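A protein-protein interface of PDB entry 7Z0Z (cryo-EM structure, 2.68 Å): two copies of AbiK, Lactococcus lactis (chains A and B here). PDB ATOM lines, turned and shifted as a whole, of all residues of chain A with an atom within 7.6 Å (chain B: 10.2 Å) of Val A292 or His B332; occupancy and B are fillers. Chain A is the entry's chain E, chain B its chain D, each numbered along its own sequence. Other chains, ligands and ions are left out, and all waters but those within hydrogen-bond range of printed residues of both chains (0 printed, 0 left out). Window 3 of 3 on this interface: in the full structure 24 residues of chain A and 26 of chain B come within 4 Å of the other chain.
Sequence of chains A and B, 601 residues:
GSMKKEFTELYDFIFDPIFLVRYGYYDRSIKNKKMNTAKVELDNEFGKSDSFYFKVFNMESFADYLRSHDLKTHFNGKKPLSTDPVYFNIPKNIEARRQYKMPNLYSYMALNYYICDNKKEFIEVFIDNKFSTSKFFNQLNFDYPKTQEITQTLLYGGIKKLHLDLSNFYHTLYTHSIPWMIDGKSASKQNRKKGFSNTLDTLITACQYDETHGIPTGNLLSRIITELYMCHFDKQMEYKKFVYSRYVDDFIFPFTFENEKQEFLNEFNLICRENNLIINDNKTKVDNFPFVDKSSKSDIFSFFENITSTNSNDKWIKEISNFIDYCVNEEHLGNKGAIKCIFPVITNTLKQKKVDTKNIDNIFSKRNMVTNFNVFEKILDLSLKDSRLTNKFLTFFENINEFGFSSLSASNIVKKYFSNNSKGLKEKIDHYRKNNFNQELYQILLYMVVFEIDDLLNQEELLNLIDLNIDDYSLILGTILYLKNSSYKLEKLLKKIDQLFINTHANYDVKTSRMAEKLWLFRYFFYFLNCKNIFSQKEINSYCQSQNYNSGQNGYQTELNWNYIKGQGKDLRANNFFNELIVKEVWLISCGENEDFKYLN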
ATOM      1  N   LYS A 161     -31.549 -25.932  13.485  1.00  0.00           N
ATOM      2  CA  LYS A 161     -30.424 -25.884  12.562  1.00  0.00           C
ATOM      3  C   LYS A 161     -29.692 -27.211  12.586  1.00  0.00           C
ATOM      4  O   LYS A 161     -29.307 -27.691  13.655  1.00  0.00           O
ATOM      5  CB  LYS A 161     -29.452 -24.755  12.899  1.00  0.00           C
ATOM      6  CG  LYS A 161     -30.020 -23.373  12.704  1.00  0.00           C
ATOM      7  CD  LYS A 161     -28.953 -22.329  12.891  1.00  0.00           C
ATOM      8  CE  LYS A 161     -28.576 -22.153  14.333  1.00  0.00           C
ATOM      9  NZ  LYS A 161     -27.602 -21.044  14.489  1.00  0.00           N
ATOM     10  N   HIS A 163     -26.327 -29.175  11.435  1.00  0.00           N
ATOM     11  CA  HIS A 163     -24.945 -28.935  11.055  1.00  0.00           C
ATOM     12  C   HIS A 163     -24.365 -30.189  10.424  1.00  0.00           C
ATOM     13  O   HIS A 163     -24.399 -31.264  11.027  1.00  0.00           O
ATOM     14  CB  HIS A 163     -24.110 -28.525  12.266  1.00  0.00           C
ATOM     15  CG  HIS A 163     -24.474 -27.187  12.827  1.00  0.00           C
ATOM     16  ND1 HIS A 163     -25.446 -27.024  13.789  1.00  0.00           N
ATOM     17  CD2 HIS A 163     -23.998 -25.950  12.558  1.00  0.00           C
ATOM     18  CE1 HIS A 163     -25.551 -25.744  14.089  1.00  0.00           C
ATOM     19  NE2 HIS A 163     -24.683 -25.070  13.356  1.00  0.00           N
ATOM     20  N   LYS A 285     -24.894 -32.306  14.208  1.00  0.00           N
ATOM     21  CA  LYS A 285     -25.656 -31.904  15.376  1.00  0.00           C
ATOM     22  C   LYS A 285     -26.853 -31.091  14.922  1.00  0.00           C
ATOM     23  O   LYS A 285     -26.871 -30.540  13.821  1.00  0.00           O
ATOM     24  CB  LYS A 285     -24.806 -31.085  16.350  1.00  0.00           C
ATOM     25  CG  LYS A 285     -24.369 -29.752  15.781  1.00  0.00           C
ATOM     26  CD  LYS A 285     -23.564 -28.954  16.780  1.00  0.00           C
ATOM     27  CE  LYS A 285     -22.190 -29.559  16.966  1.00  0.00           C
ATOM     28  NZ  LYS A 285     -21.379 -29.456  15.719  1.00  0.00           N
ATOM     29  N   ASP A 287     -29.093 -27.891  16.329  1.00  0.00           N
ATOM     30  CA  ASP A 287     -29.328 -26.816  17.278  1.00  0.00           C
ATOM     31  C   ASP A 287     -30.816 -26.527  17.354  1.00  0.00           C
ATOM     32  O   ASP A 287     -31.469 -26.327  16.327  1.00  0.00           O
ATOM     33  CB  ASP A 287     -28.570 -25.553  16.871  1.00  0.00           C
ATOM     34  CG  ASP A 287     -27.125 -25.573  17.306  1.00  0.00           C
ATOM     35  OD1 ASP A 287     -26.604 -26.672  17.591  1.00  0.00           O
ATOM     36  OD2 ASP A 287     -26.511 -24.488  17.375  1.00  0.00           O
ATOM     37  N   ASN A 288     -31.349 -26.511  18.566  1.00  0.00           N
ATOM     38  CA  ASN A 288     -32.737 -26.154  18.808  1.00  0.00           C
ATOM     39  C   ASN A 288     -32.798 -24.737  19.353  1.00  0.00           C
ATOM     40  O   ASN A 288     -31.965 -24.341  20.169  1.00  0.00           O
ATOM     41  CB  ASN A 288     -33.385 -27.121  19.796  1.00  0.00           C
ATOM     42  CG  ASN A 288     -33.448 -28.533  19.269  1.00  0.00           C
ATOM     43  OD1 ASN A 288     -34.137 -28.812  18.292  1.00  0.00           O
ATOM     44  ND2 ASN A 288     -32.727 -29.433  19.911  1.00  0.00           N
ATOM     45  N   PHE A 289     -33.778 -23.974  18.891  1.00  0.00           N
ATOM     46  CA  PHE A 289     -33.928 -22.610  19.364  1.00  0.00           C
ATOM     47  C   PHE A 289     -34.423 -22.616  20.810  1.00  0.00           C
ATOM     48  O   PHE A 289     -35.292 -23.416  21.166  1.00  0.00           O
ATOM     49  CB  PHE A 289     -34.889 -21.846  18.456  1.00  0.00           C
ATOM     50  CG  PHE A 289     -35.102 -20.415  18.847  1.00  0.00           C
ATOM     51  CD1 PHE A 289     -36.086 -20.064  19.751  1.00  0.00           C
ATOM     52  CD2 PHE A 289     -34.303 -19.424  18.321  1.00  0.00           C
ATOM     53  CE1 PHE A 289     -36.278 -18.752  20.104  1.00  0.00           C
ATOM     54  CE2 PHE A 289     -34.490 -18.108  18.676  1.00  0.00           C
ATOM     55  CZ  PHE A 289     -35.477 -17.773  19.568  1.00  0.00           C
ATOM     56  N   PRO A 290     -33.887 -21.738  21.677  1.00  0.00           N
ATOM     57  CA  PRO A 290     -32.906 -20.679  21.405  1.00  0.00           C
ATOM     58  C   PRO A 290     -31.512 -21.193  21.068  1.00  0.00           C
ATOM     59  O   PRO A 290     -31.014 -22.132  21.679  1.00  0.00           O
ATOM     60  CB  PRO A 290     -32.890 -19.887  22.710  1.00  0.00           C
ATOM     61  CG  PRO A 290     -33.334 -20.847  23.730  1.00  0.00           C
ATOM     62  CD  PRO A 290     -34.357 -21.688  23.068  1.00  0.00           C
ATOM     63  N   PHE A 291     -30.892 -20.548  20.089  1.00  0.00           N
ATOM     64  CA  PHE A 291     -29.683 -21.051  19.460  1.00  0.00           C
ATOM     65  C   PHE A 291     -28.448 -20.685  20.270  1.00  0.00           C
ATOM     66  O   PHE A 291     -28.371 -19.618  20.879  1.00  0.00           O
ATOM     67  CB  PHE A 291     -29.562 -20.487  18.047  1.00  0.00           C
ATOM     68  CG  PHE A 291     -30.552 -21.061  17.084  1.00  0.00           C
ATOM     69  CD1 PHE A 291     -30.826 -22.412  17.077  1.00  0.00           C
ATOM     70  CD2 PHE A 291     -31.198 -20.250  16.174  1.00  0.00           C
ATOM     71  CE1 PHE A 291     -31.731 -22.939  16.192  1.00  0.00           C
ATOM     72  CE2 PHE A 291     -32.107 -20.776  15.288  1.00  0.00           C
ATOM     73  CZ  PHE A 291     -32.371 -22.121  15.298  1.00  0.00           C
ATOM     74  N   VAL A 292     -27.480 -21.580  20.263  1.00  0.00           N
ATOM     75  CA  VAL A 292     -26.207 -21.355  20.934  1.00  0.00           C
ATOM     76  C   VAL A 292     -25.287 -20.580  20.003  1.00  0.00           C
ATOM     77  O   VAL A 292     -25.287 -20.785  18.784  1.00  0.00           O
ATOM     78  CB  VAL A 292     -25.580 -22.690  21.380  1.00  0.00           C
ATOM     79  CG1 VAL A 292     -25.046 -23.463  20.197  1.00  0.00           C
ATOM     80  CG2 VAL A 292     -24.478 -22.444  22.392  1.00  0.00           C
ATOM     81  N   ASP A 293     -24.531 -19.642  20.575  1.00  0.00           N
ATOM     82  CA  ASP A 293     -23.549 -18.851  19.828  1.00  0.00           C
ATOM     83  C   ASP A 293     -22.309 -18.724  20.711  1.00  0.00           C
ATOM     84  O   ASP A 293     -22.181 -17.772  21.483  1.00  0.00           O
ATOM     85  CB  ASP A 293     -24.112 -17.490  19.446  1.00  0.00           C
ATOM     86  CG  ASP A 293     -23.176 -16.701  18.553  1.00  0.00           C
ATOM     87  OD1 ASP A 293     -22.181 -17.281  18.070  1.00  0.00           O
ATOM     88  OD2 ASP A 293     -23.439 -15.504  18.325  1.00  0.00           O
ATOM     89  N   LYS A 294     -21.398 -19.688  20.586  1.00  0.00           N
ATOM     90  CA  LYS A 294     -20.169 -19.637  21.370  1.00  0.00           C
ATOM     91  C   LYS A 294     -19.182 -18.621  20.812  1.00  0.00           C
ATOM     92  O   LYS A 294     -18.512 -17.922  21.578  1.00  0.00           O
ATOM     93  CB  LYS A 294     -19.522 -21.019  21.431  1.00  0.00           C
ATOM     94  CG  LYS A 294     -20.258 -22.012  22.302  1.00  0.00           C
ATOM     95  CD  LYS A 294     -19.630 -23.386  22.198  1.00  0.00           C
ATOM     96  CE  LYS A 294     -20.585 -24.466  22.665  1.00  0.00           C
ATOM     97  NZ  LYS A 294     -20.488 -24.680  24.134  1.00  0.00           N
ATOM     98  N   SER A 295     -19.078 -18.524  19.487  1.00  0.00           N
ATOM     99  CA  SER A 295     -18.045 -17.710  18.847  1.00  0.00           C
ATOM    100  C   SER A 295     -18.534 -16.270  18.722  1.00  0.00           C
ATOM    101  O   SER A 295     -18.918 -15.795  17.654  1.00  0.00           O
ATOM    102  CB  SER A 295     -17.669 -18.300  17.496  1.00  0.00           C
ATOM    103  OG  SER A 295     -17.409 -19.686  17.607  1.00  0.00           O
ATOM    104  N   ILE B  94     -40.504 -25.449  22.929  1.00  0.00           N
ATOM    105  CA  ILE B  94     -40.385 -25.820  21.524  1.00  0.00           C
ATOM    106  C   ILE B  94     -41.179 -27.086  21.208  1.00  0.00           C
ATOM    107  O   ILE B  94     -41.460 -27.362  20.037  1.00  0.00           O
ATOM    108  CB  ILE B  94     -38.900 -25.982  21.143  1.00  0.00           C
ATOM    109  CG1 ILE B  94     -38.733 -26.110  19.625  1.00  0.00           C
ATOM    110  CG2 ILE B  94     -38.299 -27.186  21.846  1.00  0.00           C
ATOM    111  CD1 ILE B  94     -37.309 -25.952  19.146  1.00  0.00           C
ATOM    112  N   LYS B 294     -28.361 -18.301  37.078  1.00  0.00           N
ATOM    113  CA  LYS B 294     -28.273 -18.206  35.626  1.00  0.00           C
ATOM    114  C   LYS B 294     -28.984 -16.969  35.096  1.00  0.00           C
ATOM    115  O   LYS B 294     -28.495 -16.323  34.163  1.00  0.00           O
ATOM    116  CB  LYS B 294     -28.848 -19.461  34.977  1.00  0.00           C
ATOM    117  CG  LYS B 294     -27.986 -20.694  35.134  1.00  0.00           C
ATOM    118  CD  LYS B 294     -28.691 -21.916  34.584  1.00  0.00           C
ATOM    119  CE  LYS B 294     -28.087 -23.194  35.128  1.00  0.00           C
ATOM    120  NZ  LYS B 294     -26.936 -23.648  34.302  1.00  0.00           N
ATOM    121  N   SER B 295     -30.134 -16.622  35.672  1.00  0.00           N
ATOM    122  CA  SER B 295     -30.983 -15.560  35.134  1.00  0.00           C
ATOM    123  C   SER B 295     -30.525 -14.212  35.682  1.00  0.00           C
ATOM    124  O   SER B 295     -31.139 -13.619  36.569  1.00  0.00           O
ATOM    125  CB  SER B 295     -32.445 -15.835  35.458  1.00  0.00           C
ATOM    126  OG  SER B 295     -32.793 -17.164  35.118  1.00  0.00           O
ATOM    127  N   LYS B 297     -29.445 -10.383  34.203  1.00  0.00           N
ATOM    128  CA  LYS B 297     -29.680  -9.582  33.010  1.00  0.00           C
ATOM    129  C   LYS B 297     -28.718  -8.404  32.896  1.00  0.00           C
ATOM    130  O   LYS B 297     -28.958  -7.493  32.100  1.00  0.00           O
ATOM    131  CB  LYS B 297     -31.120  -9.079  32.996  1.00  0.00           C
ATOM    132  CG  LYS B 297     -32.176 -10.168  33.000  1.00  0.00           C
ATOM    133  CD  LYS B 297     -32.157 -10.994  31.738  1.00  0.00           C
ATOM    134  CE  LYS B 297     -33.331 -11.949  31.718  1.00  0.00           C
ATOM    135  NZ  LYS B 297     -33.195 -13.010  32.746  1.00  0.00           N
ATOM    136  N   ILE B 300     -27.004  -8.060  29.357  1.00  0.00           N
ATOM    137  CA  ILE B 300     -27.958  -7.656  28.330  1.00  0.00           C
ATOM    138  C   ILE B 300     -28.236  -6.162  28.414  1.00  0.00           C
ATOM    139  O   ILE B 300     -28.223  -5.453  27.402  1.00  0.00           O
ATOM    140  CB  ILE B 300     -29.252  -8.480  28.450  1.00  0.00           C
ATOM    141  CG1 ILE B 300     -28.921  -9.970  28.513  1.00  0.00           C
ATOM    142  CG2 ILE B 300     -30.212  -8.149  27.330  1.00  0.00           C
ATOM    143  CD1 ILE B 300     -30.116 -10.849  28.718  1.00  0.00           C
ATOM    144  N   ILE B 324     -28.864  -9.390  19.260  1.00  0.00           N
ATOM    145  CA  ILE B 324     -29.907 -10.404  19.132  1.00  0.00           C
ATOM    146  C   ILE B 324     -29.306 -11.795  19.267  1.00  0.00           C
ATOM    147  O   ILE B 324     -29.838 -12.655  19.981  1.00  0.00           O
ATOM    148  CB  ILE B 324     -30.664 -10.240  17.803  1.00  0.00           C
ATOM    149  CG1 ILE B 324     -31.408  -8.908  17.766  1.00  0.00           C
ATOM    150  CG2 ILE B 324     -31.625 -11.387  17.592  1.00  0.00           C
ATOM    151  CD1 ILE B 324     -31.562  -8.350  16.382  1.00  0.00           C
ATOM    152  N   ASP B 325     -28.177 -12.033  18.594  1.00  0.00           N
ATOM    153  CA  ASP B 325     -27.521 -13.333  18.724  1.00  0.00           C
ATOM    154  C   ASP B 325     -27.099 -13.596  20.165  1.00  0.00           C
ATOM    155  O   ASP B 325     -27.252 -14.714  20.676  1.00  0.00           O
ATOM    156  CB  ASP B 325     -26.318 -13.406  17.790  1.00  0.00           C
ATOM    157  CG  ASP B 325     -26.688 -13.136  16.348  1.00  0.00           C
ATOM    158  OD1 ASP B 325     -27.763 -13.599  15.916  1.00  0.00           O
ATOM    159  OD2 ASP B 325     -25.905 -12.464  15.647  1.00  0.00           O
ATOM    160  N   TYR B 326     -26.584 -12.569  20.839  1.00  0.00           N
ATOM    161  CA  TYR B 326     -26.152 -12.698  22.224  1.00  0.00           C
ATOM    162  C   TYR B 326     -27.314 -13.070  23.135  1.00  0.00           C
ATOM    163  O   TYR B 326     -27.176 -13.925  24.016  1.00  0.00           O
ATOM    164  CB  TYR B 326     -25.509 -11.386  22.670  1.00  0.00           C
ATOM    165  CG  TYR B 326     -24.940 -11.401  24.062  1.00  0.00           C
ATOM    166  CD1 TYR B 326     -23.640 -11.815  24.291  1.00  0.00           C
ATOM    167  CD2 TYR B 326     -25.703 -11.006  25.149  1.00  0.00           C
ATOM    168  CE1 TYR B 326     -23.116 -11.832  25.559  1.00  0.00           C
ATOM    169  CE2 TYR B 326     -25.185 -11.019  26.420  1.00  0.00           C
ATOM    170  CZ  TYR B 326     -23.890 -11.434  26.619  1.00  0.00           C
ATOM    171  OH  TYR B 326     -23.364 -11.453  27.887  1.00  0.00           O
ATOM    172  N   CYS B 327     -28.468 -12.439  22.937  1.00  0.00           N
ATOM    173  CA  CYS B 327     -29.613 -12.725  23.796  1.00  0.00           C
ATOM    174  C   CYS B 327     -30.194 -14.103  23.523  1.00  0.00           C
ATOM    175  O   CYS B 327     -30.656 -14.777  24.451  1.00  0.00           O
ATOM    176  CB  CYS B 327     -30.683 -11.663  23.614  1.00  0.00           C
ATOM    177  SG  CYS B 327     -30.358 -10.146  24.472  1.00  0.00           S
ATOM    178  N   VAL B 328     -30.203 -14.539  22.261  1.00  0.00           N
ATOM    179  CA  VAL B 328     -30.652 -15.899  21.980  1.00  0.00           C
ATOM    180  C   VAL B 328     -29.721 -16.912  22.637  1.00  0.00           C
ATOM    181  O   VAL B 328     -30.171 -17.910  23.214  1.00  0.00           O
ATOM    182  CB  VAL B 328     -30.779 -16.132  20.465  1.00  0.00           C
ATOM    183  CG1 VAL B 328     -31.370 -17.486  20.205  1.00  0.00           C
ATOM    184  CG2 VAL B 328     -31.684 -15.087  19.859  1.00  0.00           C
ATOM    185  N   ASN B 329     -28.411 -16.661  22.584  1.00  0.00           N
ATOM    186  CA  ASN B 329     -27.474 -17.523  23.300  1.00  0.00           C
ATOM    187  C   ASN B 329     -27.734 -17.516  24.799  1.00  0.00           C
ATOM    188  O   ASN B 329     -27.680 -18.565  25.450  1.00  0.00           O
ATOM    189  CB  ASN B 329     -26.040 -17.092  23.017  1.00  0.00           C
ATOM    190  CG  ASN B 329     -25.031 -18.067  23.566  1.00  0.00           C
ATOM    191  OD1 ASN B 329     -25.111 -19.263  23.308  1.00  0.00           O
ATOM    192  ND2 ASN B 329     -24.058 -17.559  24.304  1.00  0.00           N
ATOM    193  N   GLU B 330     -27.996 -16.339  25.370  1.00  0.00           N
ATOM    194  CA  GLU B 330     -28.247 -16.255  26.802  1.00  0.00           C
ATOM    195  C   GLU B 330     -29.483 -17.055  27.186  1.00  0.00           C
ATOM    196  O   GLU B 330     -29.481 -17.773  28.190  1.00  0.00           O
ATOM    197  CB  GLU B 330     -28.403 -14.796  27.218  1.00  0.00           C
ATOM    198  CG  GLU B 330     -27.099 -14.085  27.520  1.00  0.00           C
ATOM    199  CD  GLU B 330     -26.200 -14.860  28.462  1.00  0.00           C
ATOM    200  OE1 GLU B 330     -26.301 -14.651  29.688  1.00  0.00           O
ATOM    201  OE2 GLU B 330     -25.374 -15.663  27.978  1.00  0.00           O
ATOM    202  N   GLU B 331     -30.545 -16.949  26.388  1.00  0.00           N
ATOM    203  CA  GLU B 331     -31.737 -17.759  26.619  1.00  0.00           C
ATOM    204  C   GLU B 331     -31.415 -19.243  26.531  1.00  0.00           C
ATOM    205  O   GLU B 331     -31.923 -20.045  27.320  1.00  0.00           O
ATOM    206  CB  GLU B 331     -32.815 -17.394  25.603  1.00  0.00           C
ATOM    207  CG  GLU B 331     -34.123 -18.142  25.767  1.00  0.00           C
ATOM    208  CD  GLU B 331     -34.834 -17.814  27.055  1.00  0.00           C
ATOM    209  OE1 GLU B 331     -34.620 -16.707  27.587  1.00  0.00           O
ATOM    210  OE2 GLU B 331     -35.617 -18.661  27.535  1.00  0.00           O
ATOM    211  N   HIS B 332     -30.580 -19.626  25.565  1.00  0.00           N
ATOM    212  CA  HIS B 332     -30.183 -21.023  25.440  1.00  0.00           C
ATOM    213  C   HIS B 332     -29.411 -21.506  26.661  1.00  0.00           C
ATOM    214  O   HIS B 332     -29.544 -22.667  27.059  1.00  0.00           O
ATOM    215  CB  HIS B 332     -29.346 -21.207  24.175  1.00  0.00           C
ATOM    216  CG  HIS B 332     -28.604 -22.503  24.121  1.00  0.00           C
ATOM    217  ND1 HIS B 332     -29.190 -23.678  23.705  1.00  0.00           N
ATOM    218  CD2 HIS B 332     -27.320 -22.808  24.419  1.00  0.00           C
ATOM    219  CE1 HIS B 332     -28.301 -24.652  23.758  1.00  0.00           C
ATOM    220  NE2 HIS B 332     -27.158 -24.151  24.187  1.00  0.00           N
ATOM    221  N   LEU B 333     -28.607 -20.637  27.268  1.00  0.00           N
ATOM    222  CA  LEU B 333     -27.770 -21.005  28.401  1.00  0.00           C
ATOM    223  C   LEU B 333     -28.521 -21.024  29.725  1.00  0.00           C
ATOM    224  O   LEU B 333     -27.883 -21.128  30.776  1.00  0.00           O
ATOM    225  CB  LEU B 333     -26.578 -20.054  28.507  1.00  0.00           C
ATOM    226  CG  LEU B 333     -25.491 -20.223  27.452  1.00  0.00           C
ATOM    227  CD1 LEU B 333     -24.309 -19.327  27.760  1.00  0.00           C
ATOM    228  CD2 LEU B 333     -25.058 -21.667  27.364  1.00  0.00           C
ATOM    229  N   GLY B 334     -29.844 -20.924  29.711  1.00  0.00           N
ATOM    230  CA  GLY B 334     -30.625 -20.991  30.925  1.00  0.00           C
ATOM    231  C   GLY B 334     -31.073 -19.661  31.481  1.00  0.00           C
ATOM    232  O   GLY B 334     -31.773 -19.642  32.500  1.00  0.00           O
ATOM    233  N   ASN B 335     -30.696 -18.553  30.854  1.00  0.00           N
ATOM    234  CA  ASN B 335     -31.105 -17.225  31.303  1.00  0.00           C
ATOM    235  C   ASN B 335     -32.538 -17.003  30.838  1.00  0.00           C
ATOM    236  O   ASN B 335     -32.787 -16.478  29.754  1.00  0.00           O
ATOM    237  CB  ASN B 335     -30.152 -16.169  30.764  1.00  0.00           C
ATOM    238  CG  ASN B 335     -30.371 -14.811  31.376  1.00  0.00           C
ATOM    239  OD1 ASN B 335     -31.403 -14.546  31.983  1.00  0.00           O
ATOM    240  ND2 ASN B 335     -29.390 -13.936  31.222  1.00  0.00           N
ATOM    241  N   LYS B 336     -33.492 -17.414  31.671  1.00  0.00           N
ATOM    242  CA  LYS B 336     -34.901 -17.344  31.304  1.00  0.00           C
ATOM    243  C   LYS B 336     -35.327 -15.912  31.017  1.00  0.00           C
ATOM    244  O   LYS B 336     -34.989 -14.983  31.755  1.00  0.00           O
ATOM    245  CB  LYS B 336     -35.773 -17.929  32.415  1.00  0.00           C
ATOM    246  CG  LYS B 336     -35.518 -19.395  32.751  1.00  0.00           C
ATOM    247  CD  LYS B 336     -35.994 -20.344  31.649  1.00  0.00           C
ATOM    248  CE  LYS B 336     -34.883 -20.701  30.665  1.00  0.00           C
ATOM    249  NZ  LYS B 336     -35.322 -21.705  29.661  1.00  0.00           N
ATOM    250  N   GLY B 337     -36.075 -15.742  29.933  1.00  0.00           N
ATOM    251  CA  GLY B 337     -36.598 -14.446  29.565  1.00  0.00           C
ATOM    252  C   GLY B 337     -35.617 -13.520  28.893  1.00  0.00           C
ATOM    253  O   GLY B 337     -35.907 -12.327  28.778  1.00  0.00           O
ATOM    254  N   ALA B 338     -34.468 -14.025  28.441  1.00  0.00           N
ATOM    255  CA  ALA B 338     -33.455 -13.147  27.866  1.00  0.00           C
ATOM    256  C   ALA B 338     -33.838 -12.667  26.473  1.00  0.00           C
ATOM    257  O   ALA B 338     -33.431 -11.575  26.067  1.00  0.00           O
ATOM    258  CB  ALA B 338     -32.105 -13.854  27.831  1.00  0.00           C
ATOM    259  N   ILE B 339     -34.598 -13.465  25.720  1.00  0.00           N
ATOM    260  CA  ILE B 339     -35.049 -13.024  24.404  1.00  0.00           C
ATOM    261  C   ILE B 339     -36.111 -11.940  24.532  1.00  0.00           C
ATOM    262  O   ILE B 339     -36.146 -10.991  23.742  1.00  0.00           O
ATOM    263  CB  ILE B 339     -35.548 -14.217  23.572  1.00  0.00           C
ATOM    264  CG1 ILE B 339     -34.410 -15.197  23.310  1.00  0.00           C
ATOM    265  CG2 ILE B 339     -36.133 -13.753  22.260  1.00  0.00           C
ATOM    266  CD1 ILE B 339     -34.862 -16.502  22.727  1.00  0.00           C
ATOM    267  N   LYS B 340     -36.995 -12.059  25.522  1.00  0.00           N
ATOM    268  CA  LYS B 340     -38.035 -11.052  25.694  1.00  0.00           C
ATOM    269  C   LYS B 340     -37.465  -9.690  26.055  1.00  0.00           C
ATOM    270  O   LYS B 340     -38.171  -8.686  25.935  1.00  0.00           O
ATOM    271  CB  LYS B 340     -39.029 -11.498  26.763  1.00  0.00           C
ATOM    272  CG  LYS B 340     -39.434 -12.948  26.658  1.00  0.00           C
ATOM    273  CD  LYS B 340     -40.805 -13.166  27.252  1.00  0.00           C
ATOM    274  CE  LYS B 340     -41.884 -12.798  26.250  1.00  0.00           C
ATOM    275  NZ  LYS B 340     -43.143 -13.551  26.481  1.00  0.00           N
ATOM    276  N   ILE B 342     -34.944  -8.403  24.396  1.00  0.00           N
ATOM    277  CA  ILE B 342     -34.301  -7.863  23.197  1.00  0.00           C
ATOM    278  C   ILE B 342     -34.963  -6.556  22.782  1.00  0.00           C
ATOM    279  O   ILE B 342     -34.329  -5.495  22.748  1.00  0.00           O
ATOM    280  CB  ILE B 342     -34.344  -8.896  22.059  1.00  0.00           C
ATOM    281  CG1 ILE B 342     -33.415 -10.061  22.367  1.00  0.00           C
ATOM    282  CG2 ILE B 342     -33.962  -8.263  20.742  1.00  0.00           C
ATOM    283  CD1 ILE B 342     -33.197 -10.999  21.218  1.00  0.00           C
ATOM    284  N   LEU B 382     -36.836 -13.548  14.141  1.00  0.00           N
ATOM    285  CA  LEU B 382     -36.764 -13.922  15.547  1.00  0.00           C
ATOM    286  C   LEU B 382     -38.149 -13.990  16.172  1.00  0.00           C
ATOM    287  O   LEU B 382     -38.460 -14.929  16.910  1.00  0.00           O
ATOM    288  CB  LEU B 382     -35.900 -12.926  16.309  1.00  0.00           C
ATOM    289  CG  LEU B 382     -35.743 -13.253  17.788  1.00  0.00           C
ATOM    290  CD1 LEU B 382     -34.944 -14.523  17.977  1.00  0.00           C
ATOM    291  CD2 LEU B 382     -35.103 -12.096  18.495  1.00  0.00           C
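N of Asn B329 lies close to O of Phe A291 (3.4 Å). O of Pro A290 lies within hydrogen-bond range of ND1 of His B332, 3.1 Å away. The backbone carbonyl oxygen (O) of Phe A291 sits close to the backbone carbonyl oxygen (O) of Val B328, at 3.4 Å. N of Asp A293 lies within hydrogen-bond range of OD1 of Asn B329 (2.8 Å).
N of Ala B338 is in hydrogen-bond range of OE1 of Glu B331 (2.8 Å). The side-chain carboxylate (OE1) of Glu B331 is in hydrogen-bond range of the backbone NH (N) of Gly B337 (2.9 Å). OE2 of Glu B331 lies within salt-bridge range of NZ of Lys B336, 3.7 Å away.
Among the printed residues, pairs that only touch across the chains: Val A292 with Asn B329, Pro A290 with Val B328, Phe A289 with Ile B339, Pro A290 with Glu B331, Val A292 with His B332, Phe A289 with Val B328, Asp A293 with Asp B325, Phe A289 with Leu B382, Phe A291 with His B332, Phe A289 with Ile B94 and Pro A290 with Ile B339.
Of the printed residues of chain B, Pro A290 touches Val B328, Glu B331, His B332 and Ile B339. Printed residues of chain B within 4 Å of Phe A291: Val B328 (3.1 Å), Asn B329 (3.3 Å) and His B332 (3.8 Å). Val A292 touches just these residues of chain B: Asn B329 (3.3 Å) and His B332 (3.5 Å). Asp A293 touches two residues of chain B. Of the printed residues of chain A, Val B328 touches Phe A289, Pro A290 and Phe A291. Of the printed residues of chain A, Asn B329 touches Phe A291 (3.3 Å), Val A292 (3.3 Å) and Asp A293 (2.8 Å). His B332 touches three residues of chain A. Ala B338 touches none of the printed residues of chain A. Printed residues of chain A within 4 Å of Leu B382: Phe A289. The nearest residue of chain B that does not touch Val A292 is Leu B333 (5.1 Å). The nearest residue of chain A that does not touch His B332 is Asn A288 (4.5 Å).
Of the 12 printed residues of chain A, 5 touch a printed residue of chain B. Hydrophobic or aromatic side chains of chain A within 4 Å of the printed part of chain B: Phe A289, Pro A290 and Val A292. Hydrophobic or aromatic side chains of chain B that line the printed part of chain A: Ile B94, Val B328, His B332, Ile B339 and Leu B382. Among the printed residues, no Asp or Glu carboxylate lies within 4 Å of a Lys or Arg side-chain nitrogen of the other chain.
Positions printed for both chains: 294 and 295. Of the 15 pairs that touch across the chains among the printed residues, none has its exchanged pair printed and touching as well.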
